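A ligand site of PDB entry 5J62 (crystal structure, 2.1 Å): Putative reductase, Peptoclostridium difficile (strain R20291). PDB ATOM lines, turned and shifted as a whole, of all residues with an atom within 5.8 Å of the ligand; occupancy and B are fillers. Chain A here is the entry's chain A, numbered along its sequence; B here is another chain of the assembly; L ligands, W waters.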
ATOM      1  N   ARG A  17     -11.857  -3.321  -6.976  1.00  0.00           N
ATOM      2  CA  ARG A  17     -12.157  -4.636  -6.434  1.00  0.00           C
ATOM      3  C   ARG A  17     -12.338  -5.658  -7.527  1.00  0.00           C
ATOM      4  O   ARG A  17     -13.031  -5.393  -8.486  1.00  0.00           O
ATOM      5  CB  ARG A  17     -13.405  -4.564  -5.562  1.00  0.00           C
ATOM      6  CG  ARG A  17     -13.870  -5.896  -4.900  1.00  0.00           C
ATOM      7  CD  ARG A  17     -15.384  -6.008  -5.003  1.00  0.00           C
ATOM      8  NE  ARG A  17     -15.859  -5.865  -6.351  1.00  0.00           N
ATOM      9  CZ  ARG A  17     -15.836  -6.821  -7.272  1.00  0.00           C
ATOM     10  NH1 ARG A  17     -15.371  -8.036  -6.997  1.00  0.00           N
ATOM     11  NH2 ARG A  17     -16.285  -6.569  -8.505  1.00  0.00           N
ATOM     12  N   ARG A  18     -11.800  -6.851  -7.326  1.00  0.00           N
ATOM     13  CA  ARG A  18     -12.163  -8.005  -8.111  1.00  0.00           C
ATOM     14  C   ARG A  18     -12.328  -9.234  -7.192  1.00  0.00           C
ATOM     15  O   ARG A  18     -11.810  -9.282  -6.107  1.00  0.00           O
ATOM     16  CB  ARG A  18     -11.055  -8.303  -9.185  1.00  0.00           C
ATOM     17  CG  ARG A  18     -10.910  -7.291 -10.308  1.00  0.00           C
ATOM     18  CD  ARG A  18     -12.049  -7.347 -11.314  1.00  0.00           C
ATOM     19  NE  ARG A  18     -12.189  -8.695 -11.849  1.00  0.00           N
ATOM     20  CZ  ARG A  18     -11.526  -9.176 -12.906  1.00  0.00           C
ATOM     21  NH1 ARG A  18     -10.603  -8.442 -13.559  1.00  0.00           N
ATOM     22  NH2 ARG A  18     -11.780 -10.400 -13.300  1.00  0.00           N
ATOM     23  N   SER A  19     -12.952 -10.270  -7.709  1.00  0.00           N
ATOM     24  CA  SER A  19     -13.092 -11.553  -7.019  1.00  0.00           C
ATOM     25  C   SER A  19     -11.792 -12.294  -6.987  1.00  0.00           C
ATOM     26  O   SER A  19     -11.138 -12.391  -8.038  1.00  0.00           O
ATOM     27  CB  SER A  19     -14.156 -12.462  -7.645  1.00  0.00           C
ATOM     28  OG  SER A  19     -15.437 -11.907  -7.417  1.00  0.00           O
ATOM     29  N   ARG A  21      -9.901 -15.791  -6.501  1.00  0.00           N
ATOM     30  CA  ARG A  21     -10.117 -17.171  -6.614  1.00  0.00           C
ATOM     31  C   ARG A  21      -8.832 -18.013  -6.510  1.00  0.00           C
ATOM     32  O   ARG A  21      -8.815 -19.192  -6.904  1.00  0.00           O
ATOM     33  CB  ARG A  21     -10.816 -17.397  -7.927  1.00  0.00           C
ATOM     34  CG  ARG A  21     -12.176 -16.727  -7.974  1.00  0.00           C
ATOM     35  CD  ARG A  21     -12.904 -17.215  -9.181  1.00  0.00           C
ATOM     36  NE  ARG A  21     -14.215 -16.583  -9.298  1.00  0.00           N
ATOM     37  CZ  ARG A  21     -14.462 -15.451  -9.918  1.00  0.00           C
ATOM     38  NH1 ARG A  21     -13.499 -14.762 -10.553  1.00  0.00           N
ATOM     39  NH2 ARG A  21     -15.715 -15.023  -9.977  1.00  0.00           N
ATOM     40  N   LEU A  88     -15.009 -25.591  -4.775  1.00  0.00           N
ATOM     41  CA  LEU A  88     -16.074 -24.592  -4.752  1.00  0.00           C
ATOM     42  C   LEU A  88     -15.625 -23.262  -4.086  1.00  0.00           C
ATOM     43  O   LEU A  88     -15.967 -22.190  -4.526  1.00  0.00           O
ATOM     44  CB  LEU A  88     -17.297 -25.178  -4.052  1.00  0.00           C
ATOM     45  CG  LEU A  88     -18.564 -24.320  -4.258  1.00  0.00           C
ATOM     46  CD1 LEU A  88     -19.044 -24.457  -5.698  1.00  0.00           C
ATOM     47  CD2 LEU A  88     -19.659 -24.607  -3.270  1.00  0.00           C
ATOM     48  N   TYR A  90     -12.399 -22.368  -3.650  1.00  0.00           N
ATOM     49  CA  TYR A  90     -11.095 -21.956  -4.166  1.00  0.00           C
ATOM     50  C   TYR A  90      -9.992 -22.130  -3.111  1.00  0.00           C
ATOM     51  O   TYR A  90      -9.006 -21.416  -3.121  1.00  0.00           O
ATOM     52  CB  TYR A  90     -11.195 -20.516  -4.710  1.00  0.00           C
ATOM     53  CG  TYR A  90     -12.261 -20.407  -5.802  1.00  0.00           C
ATOM     54  CD1 TYR A  90     -12.105 -21.126  -6.997  1.00  0.00           C
ATOM     55  CD2 TYR A  90     -13.383 -19.624  -5.661  1.00  0.00           C
ATOM     56  CE1 TYR A  90     -13.040 -21.077  -7.991  1.00  0.00           C
ATOM     57  CE2 TYR A  90     -14.349 -19.579  -6.663  1.00  0.00           C
ATOM     58  CZ  TYR A  90     -14.164 -20.282  -7.832  1.00  0.00           C
ATOM     59  OH  TYR A  90     -15.040 -20.315  -8.857  1.00  0.00           O
ATOM     60  N   CYS A 130     -14.124 -13.934  -2.608  1.00  0.00           N
ATOM     61  CA  CYS A 130     -15.054 -14.245  -3.653  1.00  0.00           C
ATOM     62  C   CYS A 130     -16.339 -14.729  -2.996  1.00  0.00           C
ATOM     63  O   CYS A 130     -16.288 -15.570  -2.106  1.00  0.00           O
ATOM     64  CB  CYS A 130     -14.472 -15.365  -4.523  1.00  0.00           C
ATOM     65  SG  CYS A 130     -15.431 -15.700  -6.014  1.00  0.00           S
ATOM     66  N   ILE A 131     -17.456 -14.254  -3.471  1.00  0.00           N
ATOM     67  CA  ILE A 131     -18.734 -14.703  -2.997  1.00  0.00           C
ATOM     68  C   ILE A 131     -19.049 -16.027  -3.699  1.00  0.00           C
ATOM     69  O   ILE A 131     -18.679 -16.232  -4.884  1.00  0.00           O
ATOM     70  CB  ILE A 131     -19.784 -13.628  -3.326  1.00  0.00           C
ATOM     71  CG1 ILE A 131     -19.473 -12.348  -2.599  1.00  0.00           C
ATOM     72  CG2 ILE A 131     -21.184 -14.097  -2.892  1.00  0.00           C
ATOM     73  CD1 ILE A 131     -20.097 -11.100  -3.156  1.00  0.00           C
ATOM     74  N   ILE A 132     -19.705 -16.929  -3.005  1.00  0.00           N
ATOM     75  CA  ILE A 132     -19.908 -18.276  -3.481  1.00  0.00           C
ATOM     76  C   ILE A 132     -21.359 -18.655  -3.321  1.00  0.00           C
ATOM     77  O   ILE A 132     -21.859 -18.766  -2.171  1.00  0.00           O
ATOM     78  CB  ILE A 132     -19.065 -19.340  -2.672  1.00  0.00           C
ATOM     79  CG1 ILE A 132     -17.629 -18.940  -2.442  1.00  0.00           C
ATOM     80  CG2 ILE A 132     -19.143 -20.720  -3.355  1.00  0.00           C
ATOM     81  CD1 ILE A 132     -16.711 -18.769  -3.644  1.00  0.00           C
ATOM     82  N   GLY A 133     -22.038 -18.906  -4.437  1.00  0.00           N
ATOM     83  CA  GLY A 133     -23.463 -19.215  -4.409  1.00  0.00           C
ATOM     84  C   GLY A 133     -23.703 -20.607  -3.886  1.00  0.00           C
ATOM     85  O   GLY A 133     -22.998 -21.550  -4.280  1.00  0.00           O
ATOM     86  N   PHE A 189     -25.576 -17.683   0.039  1.00  0.00           N
ATOM     87  CA  PHE A 189     -24.222 -17.729  -0.370  1.00  0.00           C
ATOM     88  C   PHE A 189     -23.264 -17.667   0.820  1.00  0.00           C
ATOM     89  O   PHE A 189     -23.643 -17.287   1.937  1.00  0.00           O
ATOM     90  CB  PHE A 189     -23.938 -16.591  -1.375  1.00  0.00           C
ATOM     91  CG  PHE A 189     -24.270 -15.219  -0.873  1.00  0.00           C
ATOM     92  CD1 PHE A 189     -25.430 -14.567  -1.296  1.00  0.00           C
ATOM     93  CD2 PHE A 189     -23.463 -14.575  -0.008  1.00  0.00           C
ATOM     94  CE1 PHE A 189     -25.754 -13.328  -0.822  1.00  0.00           C
ATOM     95  CE2 PHE A 189     -23.748 -13.296   0.478  1.00  0.00           C
ATOM     96  CZ  PHE A 189     -24.881 -12.686   0.088  1.00  0.00           C
ATOM     97  N   ARG A 204     -11.964  -3.799 -12.928  1.00  0.00           N
ATOM     98  CA  ARG A 204     -13.023  -3.845 -13.921  1.00  0.00           C
ATOM     99  C   ARG A 204     -13.109  -2.507 -14.722  1.00  0.00           C
ATOM    100  O   ARG A 204     -13.014  -1.395 -14.175  1.00  0.00           O
ATOM    101  CB  ARG A 204     -14.384  -4.104 -13.258  1.00  0.00           C
ATOM    102  CG  ARG A 204     -15.580  -4.070 -14.220  1.00  0.00           C
ATOM    103  CD  ARG A 204     -16.939  -4.190 -13.494  1.00  0.00           C
ATOM    104  NE  ARG A 204     -17.026  -5.392 -12.718  1.00  0.00           N
ATOM    105  CZ  ARG A 204     -18.024  -5.684 -11.891  1.00  0.00           C
ATOM    106  NH1 ARG A 204     -19.035  -4.793 -11.658  1.00  0.00           N
ATOM    107  NH2 ARG A 204     -17.995  -6.841 -11.243  1.00  0.00           N
ATOM    108  N   ALA B  42     -18.814  -1.007  -9.903  1.00  0.00           N
ATOM    109  CA  ALA B  42     -17.679  -1.922  -9.659  1.00  0.00           C
ATOM    110  C   ALA B  42     -18.002  -3.088  -8.730  1.00  0.00           C
ATOM    111  O   ALA B  42     -17.128  -3.905  -8.433  1.00  0.00           O
ATOM    112  CB  ALA B  42     -16.526  -1.139  -9.094  1.00  0.00           C
ATOM    113  N   ALA B  43     -19.267  -3.215  -8.333  1.00  0.00           N
ATOM    114  CA  ALA B  43     -19.647  -4.235  -7.350  1.00  0.00           C
ATOM    115  C   ALA B  43     -19.589  -5.635  -7.990  1.00  0.00           C
ATOM    116  O   ALA B  43     -19.757  -5.790  -9.194  1.00  0.00           O
ATOM    117  CB  ALA B  43     -21.074  -3.949  -6.829  1.00  0.00           C
ATOM    118  N   PRO B  44     -19.339  -6.651  -7.181  1.00  0.00           N
ATOM    119  CA  PRO B  44     -19.484  -8.005  -7.646  1.00  0.00           C
ATOM    120  C   PRO B  44     -20.915  -8.266  -8.115  1.00  0.00           C
ATOM    121  O   PRO B  44     -21.830  -7.605  -7.678  1.00  0.00           O
ATOM    122  CB  PRO B  44     -19.166  -8.868  -6.419  1.00  0.00           C
ATOM    123  CG  PRO B  44     -18.880  -7.941  -5.303  1.00  0.00           C
ATOM    124  CD  PRO B  44     -19.292  -6.559  -5.718  1.00  0.00           C
ATOM    125  N   SER B  45     -21.097  -9.233  -8.977  1.00  0.00           N
ATOM    126  CA  SER B  45     -22.447  -9.556  -9.427  1.00  0.00           C
ATOM    127  C   SER B  45     -22.557 -11.036  -9.767  1.00  0.00           C
ATOM    128  O   SER B  45     -21.667 -11.569 -10.341  1.00  0.00           O
ATOM    129  CB  SER B  45     -22.841  -8.705 -10.626  1.00  0.00           C
ATOM    130  OG  SER B  45     -23.934  -9.268 -11.344  1.00  0.00           O
ATOM    131  N   GLY B  46     -23.614 -11.694  -9.351  1.00  0.00           N
ATOM    132  CA  GLY B  46     -23.766 -13.135  -9.597  1.00  0.00           C
ATOM    133  C   GLY B  46     -23.839 -13.353 -11.141  1.00  0.00           C
ATOM    134  O   GLY B  46     -24.519 -12.609 -11.865  1.00  0.00           O
ATOM    135  N   CYS B  47     -23.015 -14.275 -11.618  1.00  0.00           N
ATOM    136  CA  CYS B  47     -22.813 -14.577 -13.061  1.00  0.00           C
ATOM    137  C   CYS B  47     -22.289 -13.419 -13.901  1.00  0.00           C
ATOM    138  O   CYS B  47     -22.398 -13.466 -15.091  1.00  0.00           O
ATOM    139  CB  CYS B  47     -24.059 -15.083 -13.773  1.00  0.00           C
ATOM    140  SG  CYS B  47     -24.965 -16.435 -13.052  1.00  0.00           S
ATOM    141  N   ASN B  48     -21.759 -12.359 -13.290  1.00  0.00           N
ATOM    142  CA  ASN B  48     -21.418 -11.143 -13.965  1.00  0.00           C
ATOM    143  C   ASN B  48     -22.542 -10.558 -14.815  1.00  0.00           C
ATOM    144  O   ASN B  48     -22.264  -9.895 -15.799  1.00  0.00           O
ATOM    145  CB  ASN B  48     -20.095 -11.303 -14.763  1.00  0.00           C
ATOM    146  CG  ASN B  48     -19.420  -9.979 -15.004  1.00  0.00           C
ATOM    147  OD1 ASN B  48     -19.560  -9.058 -14.221  1.00  0.00           O
ATOM    148  ND2 ASN B  48     -18.753  -9.848 -16.123  1.00  0.00           N
ATOM    149  N   TRP B 106     -29.620 -13.846  -8.587  1.00  0.00           N
ATOM    150  CA  TRP B 106     -28.658 -13.234  -7.701  1.00  0.00           C
ATOM    151  C   TRP B 106     -28.925 -11.737  -7.522  1.00  0.00           C
ATOM    152  O   TRP B 106     -28.374 -11.112  -6.584  1.00  0.00           O
ATOM    153  CB  TRP B 106     -27.213 -13.559  -8.131  1.00  0.00           C
ATOM    154  CG  TRP B 106     -26.910 -15.055  -8.244  1.00  0.00           C
ATOM    155  CD1 TRP B 106     -26.709 -15.755  -9.417  1.00  0.00           C
ATOM    156  CD2 TRP B 106     -26.900 -16.049  -7.183  1.00  0.00           C
ATOM    157  NE1 TRP B 106     -26.474 -17.101  -9.151  1.00  0.00           N
ATOM    158  CE2 TRP B 106     -26.591 -17.303  -7.794  1.00  0.00           C
ATOM    159  CE3 TRP B 106     -27.007 -15.987  -5.799  1.00  0.00           C
ATOM    160  CZ2 TRP B 106     -26.444 -18.463  -7.067  1.00  0.00           C
ATOM    161  CZ3 TRP B 106     -26.875 -17.143  -5.055  1.00  0.00           C
ATOM    162  CH2 TRP B 106     -26.604 -18.379  -5.684  1.00  0.00           C
ATOM    163  N   TYR B 109     -29.208  -9.565  -4.207  1.00  0.00           N
ATOM    164  CA  TYR B 109     -27.994  -9.481  -3.449  1.00  0.00           C
ATOM    165  C   TYR B 109     -27.027  -8.531  -4.127  1.00  0.00           C
ATOM    166  O   TYR B 109     -26.412  -7.701  -3.441  1.00  0.00           O
ATOM    167  CB  TYR B 109     -27.381 -10.863  -3.257  1.00  0.00           C
ATOM    168  CG  TYR B 109     -28.400 -11.910  -2.834  1.00  0.00           C
ATOM    169  CD1 TYR B 109     -29.115 -11.764  -1.684  1.00  0.00           C
ATOM    170  CD2 TYR B 109     -28.633 -13.025  -3.606  1.00  0.00           C
ATOM    171  CE1 TYR B 109     -30.059 -12.706  -1.282  1.00  0.00           C
ATOM    172  CE2 TYR B 109     -29.576 -13.987  -3.235  1.00  0.00           C
ATOM    173  CZ  TYR B 109     -30.300 -13.807  -2.078  1.00  0.00           C
ATOM    174  OH  TYR B 109     -31.221 -14.730  -1.690  1.00  0.00           O
ATOM    175  N   ASP B 110     -26.907  -8.630  -5.462  1.00  0.00           N
ATOM    176  CA  ASP B 110     -26.040  -7.750  -6.263  1.00  0.00           C
ATOM    177  C   ASP B 110     -26.380  -6.302  -5.931  1.00  0.00           C
ATOM    178  O   ASP B 110     -25.471  -5.462  -5.751  1.00  0.00           O
ATOM    179  CB  ASP B 110     -26.197  -7.889  -7.778  1.00  0.00           C
ATOM    180  CG  ASP B 110     -25.843  -9.248  -8.324  1.00  0.00           C
ATOM    181  OD1 ASP B 110     -25.316 -10.085  -7.596  1.00  0.00           O
ATOM    182  OD2 ASP B 110     -26.084  -9.468  -9.543  1.00  0.00           O
ATOM    183  N   ILE B 113     -25.136  -4.994  -2.641  1.00  0.00           N
ATOM    184  CA  ILE B 113     -23.706  -4.748  -2.684  1.00  0.00           C
ATOM    185  C   ILE B 113     -23.418  -3.463  -3.427  1.00  0.00           C
ATOM    186  O   ILE B 113     -22.651  -2.621  -2.938  1.00  0.00           O
ATOM    187  CB  ILE B 113     -22.892  -5.874  -3.317  1.00  0.00           C
ATOM    188  CG1 ILE B 113     -23.151  -7.207  -2.651  1.00  0.00           C
ATOM    189  CG2 ILE B 113     -21.413  -5.548  -3.176  1.00  0.00           C
ATOM    190  CD1 ILE B 113     -22.731  -8.401  -3.492  1.00  0.00           C
HETATM  191  N1  LIG L   1     -17.893 -16.451  -8.153  1.00  0.00           N
HETATM  192  C1  LIG L   1     -17.549 -17.748  -8.178  1.00  0.00           C
HETATM  193  O1  LIG L   1     -16.444 -18.119  -8.619  1.00  0.00           O
HETATM  194  N2  LIG L   1     -18.406 -18.711  -7.707  1.00  0.00           N
HETATM  195  C2  LIG L   1     -19.633 -18.498  -7.200  1.00  0.00           C
HETATM  196  O2  LIG L   1     -20.381 -19.316  -6.762  1.00  0.00           O
HETATM  197  C3  LIG L   1     -20.002 -17.061  -7.190  1.00  0.00           C
HETATM  198  N3  LIG L   1     -21.202 -16.769  -6.721  1.00  0.00           N
HETATM  199  C4  LIG L   1     -21.518 -15.458  -6.653  1.00  0.00           C
HETATM  200  C5  LIG L   1     -22.770 -15.114  -6.097  1.00  0.00           C
HETATM  201  C6  LIG L   1     -23.123 -13.792  -5.955  1.00  0.00           C
HETATM  202  C7  LIG L   1     -24.413 -13.435  -5.261  1.00  0.00           C
HETATM  203  C8  LIG L   1     -22.193 -12.768  -6.317  1.00  0.00           C
HETATM  204  C9  LIG L   1     -22.545 -11.312  -6.141  1.00  0.00           C
HETATM  205  C10 LIG L   1     -21.020 -13.109  -6.965  1.00  0.00           C
HETATM  206  C11 LIG L   1     -20.647 -14.457  -7.114  1.00  0.00           C
HETATM  207  N4  LIG L   1     -19.433 -14.835  -7.652  1.00  0.00           N
HETATM  208  C12 LIG L   1     -19.077 -16.121  -7.692  1.00  0.00           C
HETATM  209  C13 LIG L   1     -18.493 -13.821  -8.165  1.00  0.00           C
HETATM  210  C14 LIG L   1     -18.926 -13.321  -9.534  1.00  0.00           C
HETATM  211  O3  LIG L   1     -18.735 -14.343 -10.523  1.00  0.00           O
HETATM  212  C15 LIG L   1     -18.146 -12.073  -9.924  1.00  0.00           C
HETATM  213  O4  LIG L   1     -18.486 -10.982  -9.091  1.00  0.00           O
HETATM  214  C16 LIG L   1     -18.378 -11.668 -11.384  1.00  0.00           C
HETATM  215  O5  LIG L   1     -17.996 -12.767 -12.220  1.00  0.00           O
HETATM  216  C17 LIG L   1     -17.596 -10.454 -11.788  1.00  0.00           C
HETATM  217  O6  LIG L   1     -16.213 -10.689 -11.467  1.00  0.00           O
HETATM  218  P1  LIG L   1     -15.457  -9.675 -10.483  1.00  0.00           P
HETATM  219  O7  LIG L   1     -16.209  -9.832  -9.058  1.00  0.00           O
HETATM  220  O8  LIG L   1     -15.518  -8.203 -10.889  1.00  0.00           O
HETATM  221  O9  LIG L   1     -14.009 -10.254 -10.346  1.00  0.00           O
HETATM  222  O   HOH W   1     -15.905 -12.641 -13.897  1.00  0.00           O
HETATM  223  O   HOH W   2     -13.867 -12.458 -12.228  1.00  0.00           O
HETATM  224  O   HOH W   3     -15.132  -7.625 -13.335  1.00  0.00           O
HETATM  225  O   HOH W   4     -17.400 -21.488  -6.748  1.00  0.00           O
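The guanidinium group (NH2) of Arg 204 is in salt-bridge range of an oxygen (O8) of the ligand, at 2.8 Å. The side-chain hydroxyl (OG) of Ser 19 lies within hydrogen-bond range of an oxygen (O7) of the ligand. An oxygen (O9) of the ligand sits at hydrogen-bond distance from the backbone NH (N) of Ser 19, 2.8 Å away. NH1 of Arg 17 lies within salt-bridge range of O7 of the ligand, 2.9 Å away. OH of Tyr 90 lies within hydrogen-bond range of O1 of the ligand (2.6 Å). O of Ser 45 of chain B sits close to O4 of the ligand. NE of Arg 18 lies within salt-bridge range of O9 of the ligand, 2.8 Å away. N of Ser 45 of chain B sits at hydrogen-bond distance from O4 of the ligand, at 3.1 Å. The side-chain sulfur (SG) of Cys 130 sits at hydrogen-bond distance from a nitrogen (N1) of the ligand (3.3 Å). O2 of the ligand is in hydrogen-bond range of N of Gly 133, 2.9 Å away. The guanidinium group (NE) of Arg 21 is in hydrogen-bond range of an oxygen (O1) of the ligand (2.8 Å).
OG of Ser 45 of chain B lies within hydrogen-bond range of OD2 of Asp 110 of chain B (2.8 Å). OD1 of Asp 110 of chain B sits at hydrogen-bond distance from N of Gly 46 of chain B (2.9 Å). NH1 of Arg 204 is in hydrogen-bond range of O of Ala 43 of chain B (2.8 Å). The guanidinium group (NH2) of Arg 17 lies within hydrogen-bond range of the backbone carbonyl oxygen (O) of Ala 42 of chain B (2.8 Å). SG of Cys 130 is in hydrogen-bond range of NE of Arg 21 (3.6 Å).
A nitrogen (N3) of the ligand lies close to the backbone carbonyl oxygen of Ile 131 (3.2 Å). Merely in contact with the ligand: Asp 110 of chain B (3.4 Å), Gly 46 of chain B (3.4 Å), Asn 48 of chain B (3.4 Å), Pro 44 of chain B (3.5 Å), Ile 132 (3.5 Å), Trp 106 of chain B (3.7 Å) and Ile 113 of chain B (3.9 Å). Hydrophobic or aromatic side chains within 4 Å of the ligand: Tyr 90, Ile 131, Ile 132, Pro 44 of chain B, Trp 106 of chain B and Ile 113 of chain B. 17 residues have an atom within 4 Å of the ligand: Arg 17, Arg 18, Ser 19, Arg 21, Tyr 90, Cys 130, Ile 131, Ile 132, Gly 133, Arg 204, Pro 44 of chain B, Ser 45 of chain B, Gly 46 of chain B, Asn 48 of chain B, Trp 106 of chain B, Asp 110 of chain B and Ile 113 of chain B. The nearest printed residue that does not touch the ligand is Phe 189 (4.2 Å).
Water W3 lies within hydrogen-bond range of O8 of the ligand (2.5 Å), NE of Arg 204 (3.0 Å) and NE of Arg 18 (3.5 Å). Water W2 lies within hydrogen-bond range of the guanidinium group of Arg 21 (2.9 Å), an oxygen (O9) of the ligand (2.9 Å) and the guanidinium group of Arg 18 (3.1 Å). Water W4 lies within hydrogen-bond range of the backbone carbonyl oxygen (O) of Leu 88, a nitrogen (N2) of the ligand and the side-chain hydroxyl (OH) of Tyr 90.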
